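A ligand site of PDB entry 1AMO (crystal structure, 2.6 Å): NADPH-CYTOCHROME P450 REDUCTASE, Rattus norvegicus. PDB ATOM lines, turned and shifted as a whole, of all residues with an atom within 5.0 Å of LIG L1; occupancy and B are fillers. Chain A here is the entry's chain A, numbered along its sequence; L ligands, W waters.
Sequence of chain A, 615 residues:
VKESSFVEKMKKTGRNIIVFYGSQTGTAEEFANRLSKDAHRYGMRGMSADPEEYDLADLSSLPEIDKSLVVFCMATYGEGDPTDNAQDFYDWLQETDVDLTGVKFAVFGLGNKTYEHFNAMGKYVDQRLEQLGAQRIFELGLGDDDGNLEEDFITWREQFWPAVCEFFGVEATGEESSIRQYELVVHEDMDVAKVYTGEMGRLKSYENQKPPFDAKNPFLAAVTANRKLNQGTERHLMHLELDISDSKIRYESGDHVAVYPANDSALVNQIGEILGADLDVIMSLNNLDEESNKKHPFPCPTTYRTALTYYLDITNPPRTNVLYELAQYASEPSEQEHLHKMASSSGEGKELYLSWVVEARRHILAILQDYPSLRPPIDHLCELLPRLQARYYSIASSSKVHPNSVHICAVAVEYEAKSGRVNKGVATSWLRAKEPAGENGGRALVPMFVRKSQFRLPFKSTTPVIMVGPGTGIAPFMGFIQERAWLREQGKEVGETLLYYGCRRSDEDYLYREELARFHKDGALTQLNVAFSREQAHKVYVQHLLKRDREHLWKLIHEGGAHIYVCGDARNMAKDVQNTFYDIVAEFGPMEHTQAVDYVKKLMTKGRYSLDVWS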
ATOM      1  N   HIS A 256     -19.492  -6.269 -26.940  1.00  0.00           N
ATOM      2  CA  HIS A 256     -20.102  -4.955 -26.899  1.00  0.00           C
ATOM      3  C   HIS A 256     -21.534  -5.010 -27.376  1.00  0.00           C
ATOM      4  O   HIS A 256     -21.927  -5.928 -28.065  1.00  0.00           O
ATOM      5  CB  HIS A 256     -19.307  -3.987 -27.771  1.00  0.00           C
ATOM      6  CG  HIS A 256     -17.863  -3.862 -27.369  1.00  0.00           C
ATOM      7  ND1 HIS A 256     -17.469  -3.248 -26.199  1.00  0.00           N
ATOM      8  CD2 HIS A 256     -16.734  -4.268 -27.992  1.00  0.00           C
ATOM      9  CE1 HIS A 256     -16.156  -3.282 -26.116  1.00  0.00           C
ATOM     10  NE2 HIS A 256     -15.687  -3.889 -27.190  1.00  0.00           N
ATOM     11  N   THR A 315     -26.646  17.071 -32.480  1.00  0.00           N
ATOM     12  CA  THR A 315     -25.924  17.522 -31.305  1.00  0.00           C
ATOM     13  C   THR A 315     -24.437  17.805 -31.481  1.00  0.00           C
ATOM     14  O   THR A 315     -23.961  18.858 -31.082  1.00  0.00           O
ATOM     15  CB  THR A 315     -26.142  16.573 -30.133  1.00  0.00           C
ATOM     16  OG1 THR A 315     -25.671  15.262 -30.477  1.00  0.00           O
ATOM     17  CG2 THR A 315     -27.609  16.493 -29.796  1.00  0.00           C
ATOM     18  N   ASN A 316     -23.694  16.890 -32.095  1.00  0.00           N
ATOM     19  CA  ASN A 316     -22.270  17.111 -32.305  1.00  0.00           C
ATOM     20  C   ASN A 316     -22.031  18.398 -33.117  1.00  0.00           C
ATOM     21  O   ASN A 316     -22.833  18.748 -33.973  1.00  0.00           O
ATOM     22  CB  ASN A 316     -21.636  15.898 -32.967  1.00  0.00           C
ATOM     23  CG  ASN A 316     -21.568  14.684 -32.026  1.00  0.00           C
ATOM     24  OD1 ASN A 316     -22.182  14.658 -30.967  1.00  0.00           O
ATOM     25  ND2 ASN A 316     -20.805  13.675 -32.437  1.00  0.00           N
ATOM     26  N   ARG A 361     -18.869  23.863 -28.263  1.00  0.00           N
ATOM     27  CA  ARG A 361     -19.864  22.803 -28.392  1.00  0.00           C
ATOM     28  C   ARG A 361     -21.244  23.309 -28.799  1.00  0.00           C
ATOM     29  O   ARG A 361     -22.262  23.048 -28.148  1.00  0.00           O
ATOM     30  CB  ARG A 361     -19.911  21.955 -27.136  1.00  0.00           C
ATOM     31  CG  ARG A 361     -18.546  21.360 -26.861  1.00  0.00           C
ATOM     32  CD  ARG A 361     -18.648  19.923 -26.441  1.00  0.00           C
ATOM     33  NE  ARG A 361     -19.006  19.031 -27.536  1.00  0.00           N
ATOM     34  CZ  ARG A 361     -18.140  18.230 -28.153  1.00  0.00           C
ATOM     35  NH1 ARG A 361     -16.867  18.218 -27.782  1.00  0.00           N
ATOM     36  NH2 ARG A 361     -18.572  17.414 -29.099  1.00  0.00           N
ATOM     37  N   ARG A 391     -24.398   4.045 -30.060  1.00  0.00           N
ATOM     38  CA  ARG A 391     -23.363   4.089 -29.050  1.00  0.00           C
ATOM     39  C   ARG A 391     -23.123   2.696 -28.499  1.00  0.00           C
ATOM     40  O   ARG A 391     -24.062   1.940 -28.303  1.00  0.00           O
ATOM     41  CB  ARG A 391     -23.710   5.083 -27.947  1.00  0.00           C
ATOM     42  CG  ARG A 391     -23.510   6.539 -28.352  1.00  0.00           C
ATOM     43  CD  ARG A 391     -24.796   7.213 -28.827  1.00  0.00           C
ATOM     44  NE  ARG A 391     -24.670   7.802 -30.161  1.00  0.00           N
ATOM     45  CZ  ARG A 391     -24.551   9.105 -30.411  1.00  0.00           C
ATOM     46  NH1 ARG A 391     -24.561   9.990 -29.419  1.00  0.00           N
ATOM     47  NH2 ARG A 391     -24.400   9.531 -31.658  1.00  0.00           N
ATOM     48  N   TYR A 392     -21.853   2.362 -28.265  1.00  0.00           N
ATOM     49  CA  TYR A 392     -21.476   1.041 -27.748  1.00  0.00           C
ATOM     50  C   TYR A 392     -21.246   1.028 -26.238  1.00  0.00           C
ATOM     51  O   TYR A 392     -20.807   2.017 -25.647  1.00  0.00           O
ATOM     52  CB  TYR A 392     -20.203   0.552 -28.450  1.00  0.00           C
ATOM     53  CG  TYR A 392     -20.370   0.345 -29.927  1.00  0.00           C
ATOM     54  CD1 TYR A 392     -20.200   1.398 -30.826  1.00  0.00           C
ATOM     55  CD2 TYR A 392     -20.710  -0.908 -30.441  1.00  0.00           C
ATOM     56  CE1 TYR A 392     -20.364   1.206 -32.196  1.00  0.00           C
ATOM     57  CE2 TYR A 392     -20.878  -1.111 -31.803  1.00  0.00           C
ATOM     58  CZ  TYR A 392     -20.708  -0.045 -32.682  1.00  0.00           C
ATOM     59  OH  TYR A 392     -20.869  -0.232 -34.030  1.00  0.00           O
ATOM     60  N   TYR A 393     -21.526  -0.116 -25.623  1.00  0.00           N
ATOM     61  CA  TYR A 393     -21.367  -0.308 -24.185  1.00  0.00           C
ATOM     62  C   TYR A 393     -20.837  -1.700 -23.846  1.00  0.00           C
ATOM     63  O   TYR A 393     -21.344  -2.703 -24.346  1.00  0.00           O
ATOM     64  CB  TYR A 393     -22.710  -0.083 -23.468  1.00  0.00           C
ATOM     65  CG  TYR A 393     -23.230   1.304 -23.633  1.00  0.00           C
ATOM     66  CD1 TYR A 393     -22.724   2.341 -22.876  1.00  0.00           C
ATOM     67  CD2 TYR A 393     -24.190   1.609 -24.604  1.00  0.00           C
ATOM     68  CE1 TYR A 393     -23.130   3.649 -23.075  1.00  0.00           C
ATOM     69  CE2 TYR A 393     -24.601   2.914 -24.810  1.00  0.00           C
ATOM     70  CZ  TYR A 393     -24.055   3.924 -24.046  1.00  0.00           C
ATOM     71  OH  TYR A 393     -24.405   5.232 -24.257  1.00  0.00           O
ATOM     72  N   SER A 394     -19.801  -1.767 -23.022  1.00  0.00           N
ATOM     73  CA  SER A 394     -19.235  -3.054 -22.649  1.00  0.00           C
ATOM     74  C   SER A 394     -20.280  -3.757 -21.813  1.00  0.00           C
ATOM     75  O   SER A 394     -20.740  -3.222 -20.818  1.00  0.00           O
ATOM     76  CB  SER A 394     -17.961  -2.867 -21.847  1.00  0.00           C
ATOM     77  OG  SER A 394     -16.891  -2.434 -22.667  1.00  0.00           O
ATOM     78  N   CYS A 409     -23.538  -0.590 -18.118  1.00  0.00           N
ATOM     79  CA  CYS A 409     -23.063   0.262 -17.024  1.00  0.00           C
ATOM     80  C   CYS A 409     -22.660   1.543 -17.715  1.00  0.00           C
ATOM     81  O   CYS A 409     -21.850   1.514 -18.631  1.00  0.00           O
ATOM     82  CB  CYS A 409     -21.865  -0.351 -16.308  1.00  0.00           C
ATOM     83  SG  CYS A 409     -21.164   0.670 -14.938  1.00  0.00           S
ATOM     84  N   ALA A 410     -23.225   2.665 -17.294  1.00  0.00           N
ATOM     85  CA  ALA A 410     -22.866   3.911 -17.954  1.00  0.00           C
ATOM     86  C   ALA A 410     -23.001   5.141 -17.091  1.00  0.00           C
ATOM     87  O   ALA A 410     -23.805   5.185 -16.161  1.00  0.00           O
ATOM     88  CB  ALA A 410     -23.674   4.073 -19.229  1.00  0.00           C
ATOM     89  N   VAL A 411     -22.194   6.144 -17.411  1.00  0.00           N
ATOM     90  CA  VAL A 411     -22.249   7.417 -16.711  1.00  0.00           C
ATOM     91  C   VAL A 411     -22.951   8.378 -17.665  1.00  0.00           C
ATOM     92  O   VAL A 411     -22.584   8.499 -18.835  1.00  0.00           O
ATOM     93  CB  VAL A 411     -20.826   7.928 -16.360  1.00  0.00           C
ATOM     94  CG1 VAL A 411     -19.956   7.934 -17.599  1.00  0.00           C
ATOM     95  CG2 VAL A 411     -20.895   9.302 -15.755  1.00  0.00           C
ATOM     96  N   VAL A 413     -23.731  11.471 -19.554  1.00  0.00           N
ATOM     97  CA  VAL A 413     -23.033  12.691 -19.949  1.00  0.00           C
ATOM     98  C   VAL A 413     -23.979  13.884 -19.896  1.00  0.00           C
ATOM     99  O   VAL A 413     -25.139  13.796 -20.292  1.00  0.00           O
ATOM    100  CB  VAL A 413     -22.414  12.589 -21.343  1.00  0.00           C
ATOM    101  CG1 VAL A 413     -21.882  13.943 -21.782  1.00  0.00           C
ATOM    102  CG2 VAL A 413     -21.296  11.558 -21.337  1.00  0.00           C
ATOM    103  N   TYR A 415     -23.079  18.346 -19.234  1.00  0.00           N
ATOM    104  CA  TYR A 415     -22.157  19.366 -18.783  1.00  0.00           C
ATOM    105  C   TYR A 415     -22.602  20.724 -19.307  1.00  0.00           C
ATOM    106  O   TYR A 415     -23.573  20.816 -20.057  1.00  0.00           O
ATOM    107  CB  TYR A 415     -20.754  19.035 -19.332  1.00  0.00           C
ATOM    108  CG  TYR A 415     -20.747  18.862 -20.826  1.00  0.00           C
ATOM    109  CD1 TYR A 415     -21.202  17.685 -21.407  1.00  0.00           C
ATOM    110  CD2 TYR A 415     -20.356  19.902 -21.668  1.00  0.00           C
ATOM    111  CE1 TYR A 415     -21.284  17.537 -22.773  1.00  0.00           C
ATOM    112  CE2 TYR A 415     -20.426  19.767 -23.048  1.00  0.00           C
ATOM    113  CZ  TYR A 415     -20.894  18.590 -23.594  1.00  0.00           C
ATOM    114  OH  TYR A 415     -20.995  18.446 -24.950  1.00  0.00           O
ATOM    115  N   LYS A 424     -26.373  17.674 -23.412  1.00  0.00           N
ATOM    116  CA  LYS A 424     -26.634  16.373 -22.798  1.00  0.00           C
ATOM    117  C   LYS A 424     -26.268  15.224 -23.736  1.00  0.00           C
ATOM    118  O   LYS A 424     -26.448  15.319 -24.942  1.00  0.00           O
ATOM    119  CB  LYS A 424     -28.103  16.250 -22.379  1.00  0.00           C
ATOM    120  CG  LYS A 424     -28.603  17.318 -21.406  1.00  0.00           C
ATOM    121  CD  LYS A 424     -30.053  17.039 -20.987  1.00  0.00           C
ATOM    122  CE  LYS A 424     -30.534  18.010 -19.911  1.00  0.00           C
ATOM    123  NZ  LYS A 424     -30.495  19.427 -20.368  1.00  0.00           N
ATOM    124  N   GLY A 425     -25.737  14.132 -23.174  1.00  0.00           N
ATOM    125  CA  GLY A 425     -25.371  12.979 -23.983  1.00  0.00           C
ATOM    126  C   GLY A 425     -26.604  12.413 -24.659  1.00  0.00           C
ATOM    127  O   GLY A 425     -27.639  12.251 -24.024  1.00  0.00           O
ATOM    128  N   VAL A 426     -26.489  12.094 -25.939  1.00  0.00           N
ATOM    129  CA  VAL A 426     -27.635  11.564 -26.690  1.00  0.00           C
ATOM    130  C   VAL A 426     -28.183  10.250 -26.141  1.00  0.00           C
ATOM    131  O   VAL A 426     -29.312  10.207 -25.630  1.00  0.00           O
ATOM    132  CB  VAL A 426     -27.290  11.414 -28.196  1.00  0.00           C
ATOM    133  CG1 VAL A 426     -28.539  11.033 -28.987  1.00  0.00           C
ATOM    134  CG2 VAL A 426     -26.719  12.706 -28.739  1.00  0.00           C
ATOM    135  N   ALA A 427     -27.389   9.202 -26.200  1.00  0.00           N
ATOM    136  CA  ALA A 427     -27.802   7.887 -25.731  1.00  0.00           C
ATOM    137  C   ALA A 427     -28.026   7.781 -24.231  1.00  0.00           C
ATOM    138  O   ALA A 427     -29.013   7.198 -23.803  1.00  0.00           O
ATOM    139  CB  ALA A 427     -26.820   6.829 -26.183  1.00  0.00           C
ATOM    140  N   THR A 428     -27.091   8.321 -23.429  1.00  0.00           N
ATOM    141  CA  THR A 428     -27.159   8.294 -21.952  1.00  0.00           C
ATOM    142  C   THR A 428     -28.373   8.989 -21.348  1.00  0.00           C
ATOM    143  O   THR A 428     -28.917   8.528 -20.341  1.00  0.00           O
ATOM    144  CB  THR A 428     -25.885   8.870 -21.321  1.00  0.00           C
ATOM    145  OG1 THR A 428     -25.771  10.256 -21.664  1.00  0.00           O
ATOM    146  CG2 THR A 428     -24.656   8.114 -21.782  1.00  0.00           C
ATOM    147  N   SER A 429     -28.791  10.113 -21.923  1.00  0.00           N
ATOM    148  CA  SER A 429     -29.975  10.813 -21.443  1.00  0.00           C
ATOM    149  C   SER A 429     -31.144   9.919 -21.763  1.00  0.00           C
ATOM    150  O   SER A 429     -32.041   9.718 -20.938  1.00  0.00           O
ATOM    151  CB  SER A 429     -30.143  12.132 -22.193  1.00  0.00           C
ATOM    152  OG  SER A 429     -29.031  12.977 -21.993  1.00  0.00           O
ATOM    153  N   THR A 472     -16.225   3.611 -14.902  1.00  0.00           N
ATOM    154  CA  THR A 472     -17.175   2.783 -15.628  1.00  0.00           C
ATOM    155  C   THR A 472     -16.452   1.673 -16.355  1.00  0.00           C
ATOM    156  O   THR A 472     -17.079   0.870 -17.032  1.00  0.00           O
ATOM    157  CB  THR A 472     -17.999   3.584 -16.613  1.00  0.00           C
ATOM    158  OG1 THR A 472     -17.137   4.429 -17.380  1.00  0.00           O
ATOM    159  CG2 THR A 472     -19.039   4.417 -15.889  1.00  0.00           C
ATOM    160  N   ALA A 475     -17.326  -2.163 -15.958  1.00  0.00           N
ATOM    161  CA  ALA A 475     -18.417  -2.770 -16.716  1.00  0.00           C
ATOM    162  C   ALA A 475     -18.151  -4.215 -17.133  1.00  0.00           C
ATOM    163  O   ALA A 475     -18.729  -5.126 -16.560  1.00  0.00           O
ATOM    164  CB  ALA A 475     -18.778  -1.901 -17.917  1.00  0.00           C
ATOM    165  N   ASP A 612      -9.676  -2.420 -23.549  1.00  0.00           N
ATOM    166  CA  ASP A 612     -11.080  -2.130 -23.802  1.00  0.00           C
ATOM    167  C   ASP A 612     -11.243  -0.684 -23.353  1.00  0.00           C
ATOM    168  O   ASP A 612     -11.977  -0.383 -22.408  1.00  0.00           O
ATOM    169  CB  ASP A 612     -11.965  -3.039 -22.955  1.00  0.00           C
ATOM    170  CG  ASP A 612     -13.458  -2.764 -23.127  1.00  0.00           C
ATOM    171  OD1 ASP A 612     -13.870  -2.151 -24.140  1.00  0.00           O
ATOM    172  OD2 ASP A 612     -14.224  -3.175 -22.231  1.00  0.00           O
ATOM    173  N   TRP A 614     -11.630   3.681 -24.247  1.00  0.00           N
ATOM    174  CA  TRP A 614     -12.341   4.597 -25.113  1.00  0.00           C
ATOM    175  C   TRP A 614     -12.102   6.050 -24.752  1.00  0.00           C
ATOM    176  O   TRP A 614     -11.125   6.383 -24.087  1.00  0.00           O
ATOM    177  CB  TRP A 614     -13.842   4.270 -25.152  1.00  0.00           C
ATOM    178  CG  TRP A 614     -14.559   4.355 -23.837  1.00  0.00           C
ATOM    179  CD1 TRP A 614     -15.204   5.457 -23.328  1.00  0.00           C
ATOM    180  CD2 TRP A 614     -14.773   3.301 -22.895  1.00  0.00           C
ATOM    181  NE1 TRP A 614     -15.795   5.144 -22.130  1.00  0.00           N
ATOM    182  CE2 TRP A 614     -15.539   3.832 -21.841  1.00  0.00           C
ATOM    183  CE3 TRP A 614     -14.380   1.958 -22.840  1.00  0.00           C
ATOM    184  CZ2 TRP A 614     -15.927   3.055 -20.737  1.00  0.00           C
ATOM    185  CZ3 TRP A 614     -14.772   1.191 -21.737  1.00  0.00           C
ATOM    186  CH2 TRP A 614     -15.535   1.741 -20.706  1.00  0.00           C
ATOM    187  N   SER A 615     -12.966   6.935 -25.231  1.00  0.00           N
ATOM    188  CA  SER A 615     -12.851   8.360 -24.952  1.00  0.00           C
ATOM    189  C   SER A 615     -14.225   9.020 -24.952  1.00  0.00           C
ATOM    190  O   SER A 615     -15.224   8.305 -25.243  1.00  0.00           O
ATOM    191  CB  SER A 615     -11.949   9.025 -25.980  1.00  0.00           C
ATOM    192  OG  SER A 615     -10.682   8.388 -26.056  1.00  0.00           O
HETATM  193  P1  LIG L   1     -22.870  12.071 -26.843  1.00  0.00           P
HETATM  194  O1  LIG L   1     -24.050  12.872 -27.174  1.00  0.00           O
HETATM  195  O2  LIG L   1     -22.179  11.238 -27.838  1.00  0.00           O
HETATM  196  O3  LIG L   1     -21.805  13.107 -26.292  1.00  0.00           O
HETATM  197  C1  LIG L   1     -20.514  12.635 -26.016  1.00  0.00           C
HETATM  198  C2  LIG L   1     -19.459  13.678 -26.357  1.00  0.00           C
HETATM  199  O4  LIG L   1     -19.601  14.882 -25.594  1.00  0.00           O
HETATM  200  C3  LIG L   1     -18.082  13.181 -25.951  1.00  0.00           C
HETATM  201  O5  LIG L   1     -17.677  12.137 -26.869  1.00  0.00           O
HETATM  202  C4  LIG L   1     -17.372  14.511 -26.208  1.00  0.00           C
HETATM  203  O6  LIG L   1     -17.436  14.697 -27.646  1.00  0.00           O
HETATM  204  C5  LIG L   1     -18.315  15.481 -25.479  1.00  0.00           C
HETATM  205  N1  LIG L   1     -18.111  15.801 -23.997  1.00  0.00           N
HETATM  206  C6  LIG L   1     -18.499  15.106 -22.848  1.00  0.00           C
HETATM  207  N2  LIG L   1     -18.366  15.764 -21.710  1.00  0.00           N
HETATM  208  C7  LIG L   1     -17.825  16.988 -22.102  1.00  0.00           C
HETATM  209  C8  LIG L   1     -17.445  18.132 -21.380  1.00  0.00           C
HETATM  210  N3  LIG L   1     -17.593  18.279 -20.072  1.00  0.00           N
HETATM  211  N4  LIG L   1     -16.950  19.156 -22.082  1.00  0.00           N
HETATM  212  C9  LIG L   1     -16.829  19.061 -23.406  1.00  0.00           C
HETATM  213  N5  LIG L   1     -17.158  18.058 -24.193  1.00  0.00           N
HETATM  214  C10 LIG L   1     -17.657  17.023 -23.484  1.00  0.00           C
HETATM  215  N6  LIG L   1     -19.616   4.395 -21.787  1.00  0.00           N
HETATM  216  C11 LIG L   1     -20.065   4.065 -20.566  1.00  0.00           C
HETATM  217  O7  LIG L   1     -20.659   4.887 -19.864  1.00  0.00           O
HETATM  218  N7  LIG L   1     -19.893   2.758 -20.233  1.00  0.00           N
HETATM  219  C12 LIG L   1     -19.307   1.758 -21.025  1.00  0.00           C
HETATM  220  O8  LIG L   1     -19.223   0.613 -20.595  1.00  0.00           O
HETATM  221  C13 LIG L   1     -18.851   2.147 -22.313  1.00  0.00           C
HETATM  222  N8  LIG L   1     -18.281   1.164 -23.088  1.00  0.00           N
HETATM  223  C14 LIG L   1     -17.880   1.628 -24.304  1.00  0.00           C
HETATM  224  C15 LIG L   1     -17.234   0.693 -25.112  1.00  0.00           C
HETATM  225  C16 LIG L   1     -16.704   0.991 -26.326  1.00  0.00           C
HETATM  226  C17 LIG L   1     -15.949  -0.048 -27.102  1.00  0.00           C
HETATM  227  C18 LIG L   1     -16.809   2.290 -26.841  1.00  0.00           C
HETATM  228  C19 LIG L   1     -16.169   2.570 -28.186  1.00  0.00           C
HETATM  229  C20 LIG L   1     -17.445   3.254 -26.091  1.00  0.00           C
HETATM  230  C21 LIG L   1     -17.986   2.940 -24.799  1.00  0.00           C
HETATM  231  N9  LIG L   1     -18.586   3.890 -23.927  1.00  0.00           N
HETATM  232  C22 LIG L   1     -19.038   3.484 -22.622  1.00  0.00           C
HETATM  233  C23 LIG L   1     -18.799   5.274 -24.301  1.00  0.00           C
HETATM  234  C24 LIG L   1     -20.213   5.320 -24.883  1.00  0.00           C
HETATM  235  O9  LIG L   1     -20.262   4.564 -26.116  1.00  0.00           O
HETATM  236  C25 LIG L   1     -20.632   6.769 -25.128  1.00  0.00           C
HETATM  237  O10 LIG L   1     -19.609   7.619 -25.611  1.00  0.00           O
HETATM  238  C26 LIG L   1     -21.152   7.444 -23.880  1.00  0.00           C
HETATM  239  O11 LIG L   1     -22.157   6.621 -23.331  1.00  0.00           O
HETATM  240  C27 LIG L   1     -21.711   8.835 -24.224  1.00  0.00           C
HETATM  241  O12 LIG L   1     -22.632   8.865 -25.342  1.00  0.00           O
HETATM  242  P2  LIG L   1     -23.838   9.894 -25.427  1.00  0.00           P
HETATM  243  O13 LIG L   1     -24.663   9.639 -26.612  1.00  0.00           O
HETATM  244  O14 LIG L   1     -24.487   9.908 -24.118  1.00  0.00           O
HETATM  245  O15 LIG L   1     -23.195  11.264 -25.591  1.00  0.00           O
HETATM  246  N1  LG2 L   2      -7.425   4.892 -34.208  1.00  0.00           N
HETATM  247  C1  LG2 L   2      -6.188   4.495 -34.513  1.00  0.00           C
HETATM  248  O1  LG2 L   2      -5.415   5.241 -35.115  1.00  0.00           O
HETATM  249  N2  LG2 L   2      -5.873   3.231 -34.117  1.00  0.00           N
HETATM  250  C2  LG2 L   2      -6.688   2.338 -33.440  1.00  0.00           C
HETATM  251  O2  LG2 L   2      -6.288   1.204 -33.219  1.00  0.00           O
HETATM  252  C3  LG2 L   2      -7.988   2.830 -33.130  1.00  0.00           C
HETATM  253  N3  LG2 L   2      -8.767   1.988 -32.421  1.00  0.00           N
HETATM  254  C4  LG2 L   2      -9.958   2.554 -32.113  1.00  0.00           C
HETATM  255  C5  LG2 L   2     -10.806   1.774 -31.305  1.00  0.00           C
HETATM  256  C6  LG2 L   2     -12.007   2.233 -30.883  1.00  0.00           C
HETATM  257  C7  LG2 L   2     -12.874   1.380 -29.995  1.00  0.00           C
HETATM  258  C8  LG2 L   2     -12.413   3.507 -31.259  1.00  0.00           C
HETATM  259  C9  LG2 L   2     -13.732   4.080 -30.763  1.00  0.00           C
HETATM  260  C10 LG2 L   2     -11.637   4.263 -32.033  1.00  0.00           C
HETATM  261  C11 LG2 L   2     -10.415   3.833 -32.468  1.00  0.00           C
HETATM  262  N4  LG2 L   2      -9.570   4.627 -33.242  1.00  0.00           N
HETATM  263  C12 LG2 L   2      -8.285   4.118 -33.560  1.00  0.00           C
HETATM  264  C13 LG2 L   2     -10.063   5.900 -33.774  1.00  0.00           C
HETATM  265  C14 LG2 L   2     -10.931   5.909 -35.048  1.00  0.00           C
HETATM  266  O3  LG2 L   2     -10.281   5.325 -36.167  1.00  0.00           O
HETATM  267  C15 LG2 L   2     -11.343   7.357 -35.401  1.00  0.00           C
HETATM  268  O4  LG2 L   2     -12.321   7.849 -34.493  1.00  0.00           O
HETATM  269  C16 LG2 L   2     -11.985   7.560 -36.781  1.00  0.00           C
HETATM  270  O5  LG2 L   2     -12.354   8.933 -36.928  1.00  0.00           O
HETATM  271  C17 LG2 L   2     -13.234   6.699 -36.944  1.00  0.00           C
HETATM  272  O6  LG2 L   2     -13.895   6.843 -38.222  1.00  0.00           O
HETATM  273  P1  LG2 L   2     -15.322   6.209 -38.508  1.00  0.00           P
HETATM  274  O7  LG2 L   2     -15.363   6.182 -39.977  1.00  0.00           O
HETATM  275  O8  LG2 L   2     -16.242   7.154 -37.874  1.00  0.00           O
HETATM  276  O9  LG2 L   2     -15.228   4.874 -37.906  1.00  0.00           O
HETATM  277  O   HOH W   1     -19.140   4.535 -28.870  1.00  0.00           O
HETATM  278  O   HOH W   2     -21.126   7.393 -20.822  1.00  0.00           O
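The side-chain hydroxyl (OG1) of Thr 428 sits at hydrogen-bond distance from an oxygen (O14) of LIG L1. N of Val 426 lies within hydrogen-bond range of O1 of LIG L1. N of Thr 428 sits close to O14 of LIG L1, at 3.1 Å. O of Tyr 392 lies within hydrogen-bond range of O9 of LIG L1 (2.6 Å). The backbone NH of Ala 427 is in hydrogen-bond range of an oxygen (O13) of LIG L1 (2.8 Å). N8 of LIG L1 lies within hydrogen-bond range of N of Ser 394, at 3.3 Å. O11 of LIG L1 is in hydrogen-bond range of OH of Tyr 393, at 2.8 Å. O7 of LIG L1 is in hydrogen-bond range of N of Val 411, 3.2 Å away. An oxygen (O13) of LIG L1 lies within salt-bridge range of the guanidinium group of Arg 391. NH2 of Arg 361 lies within hydrogen-bond range of O6 of LIG L1, 3.3 Å away. A nitrogen (N7) of LIG L1 lies within hydrogen-bond range of the backbone carbonyl oxygen of Cys 409 (2.8 Å). The backbone NH (N) of Tyr 392 is in hydrogen-bond range of an oxygen (O9) of LIG L1, at 3.5 Å.
NE of Arg 361 lies close to OH of Tyr 415. The backbone carbonyl oxygen of Val 413 sits at hydrogen-bond distance from the backbone NH of Gly 425 (3.0 Å). The side-chain hydroxyl of Ser 429 lies within hydrogen-bond range of the backbone carbonyl oxygen of Gly 425, 2.6 Å away. OG1 of Thr 428 is in hydrogen-bond range of N of Val 413 (3.2 Å). OD2 of Asp 612 lies within hydrogen-bond range of OG of Ser 394 (2.8 Å).
His 256 touches LIG L1. CA of Ala 410 touches O7 of LIG L1 (3.1 Å). CG1 of Val 413 touches C6 of LIG L1, 3.7 Å away. CG of Tyr 415 touches N3 of LIG L1, 3.3 Å away. Gly 425 touches LIG L1 (CA to O14, 3.2 Å). Ala 475 touches LIG L1. CZ2 of Trp 614 touches C13 of LIG L1, at 3.4 Å. Hydrophobic or aromatic side chains that line LIG L1: His 256, Tyr 393, Ala 410, Val 411, Val 413, Tyr 415, Val 426, Ala 427, Ala 475 and Trp 614. The nearest printed residue that does not touch LIG L1 is Lys 424 (4.1 Å).
Water W2 bridges the backbone carbonyl oxygen of Val 411 and an oxygen (O7) of LIG L1.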
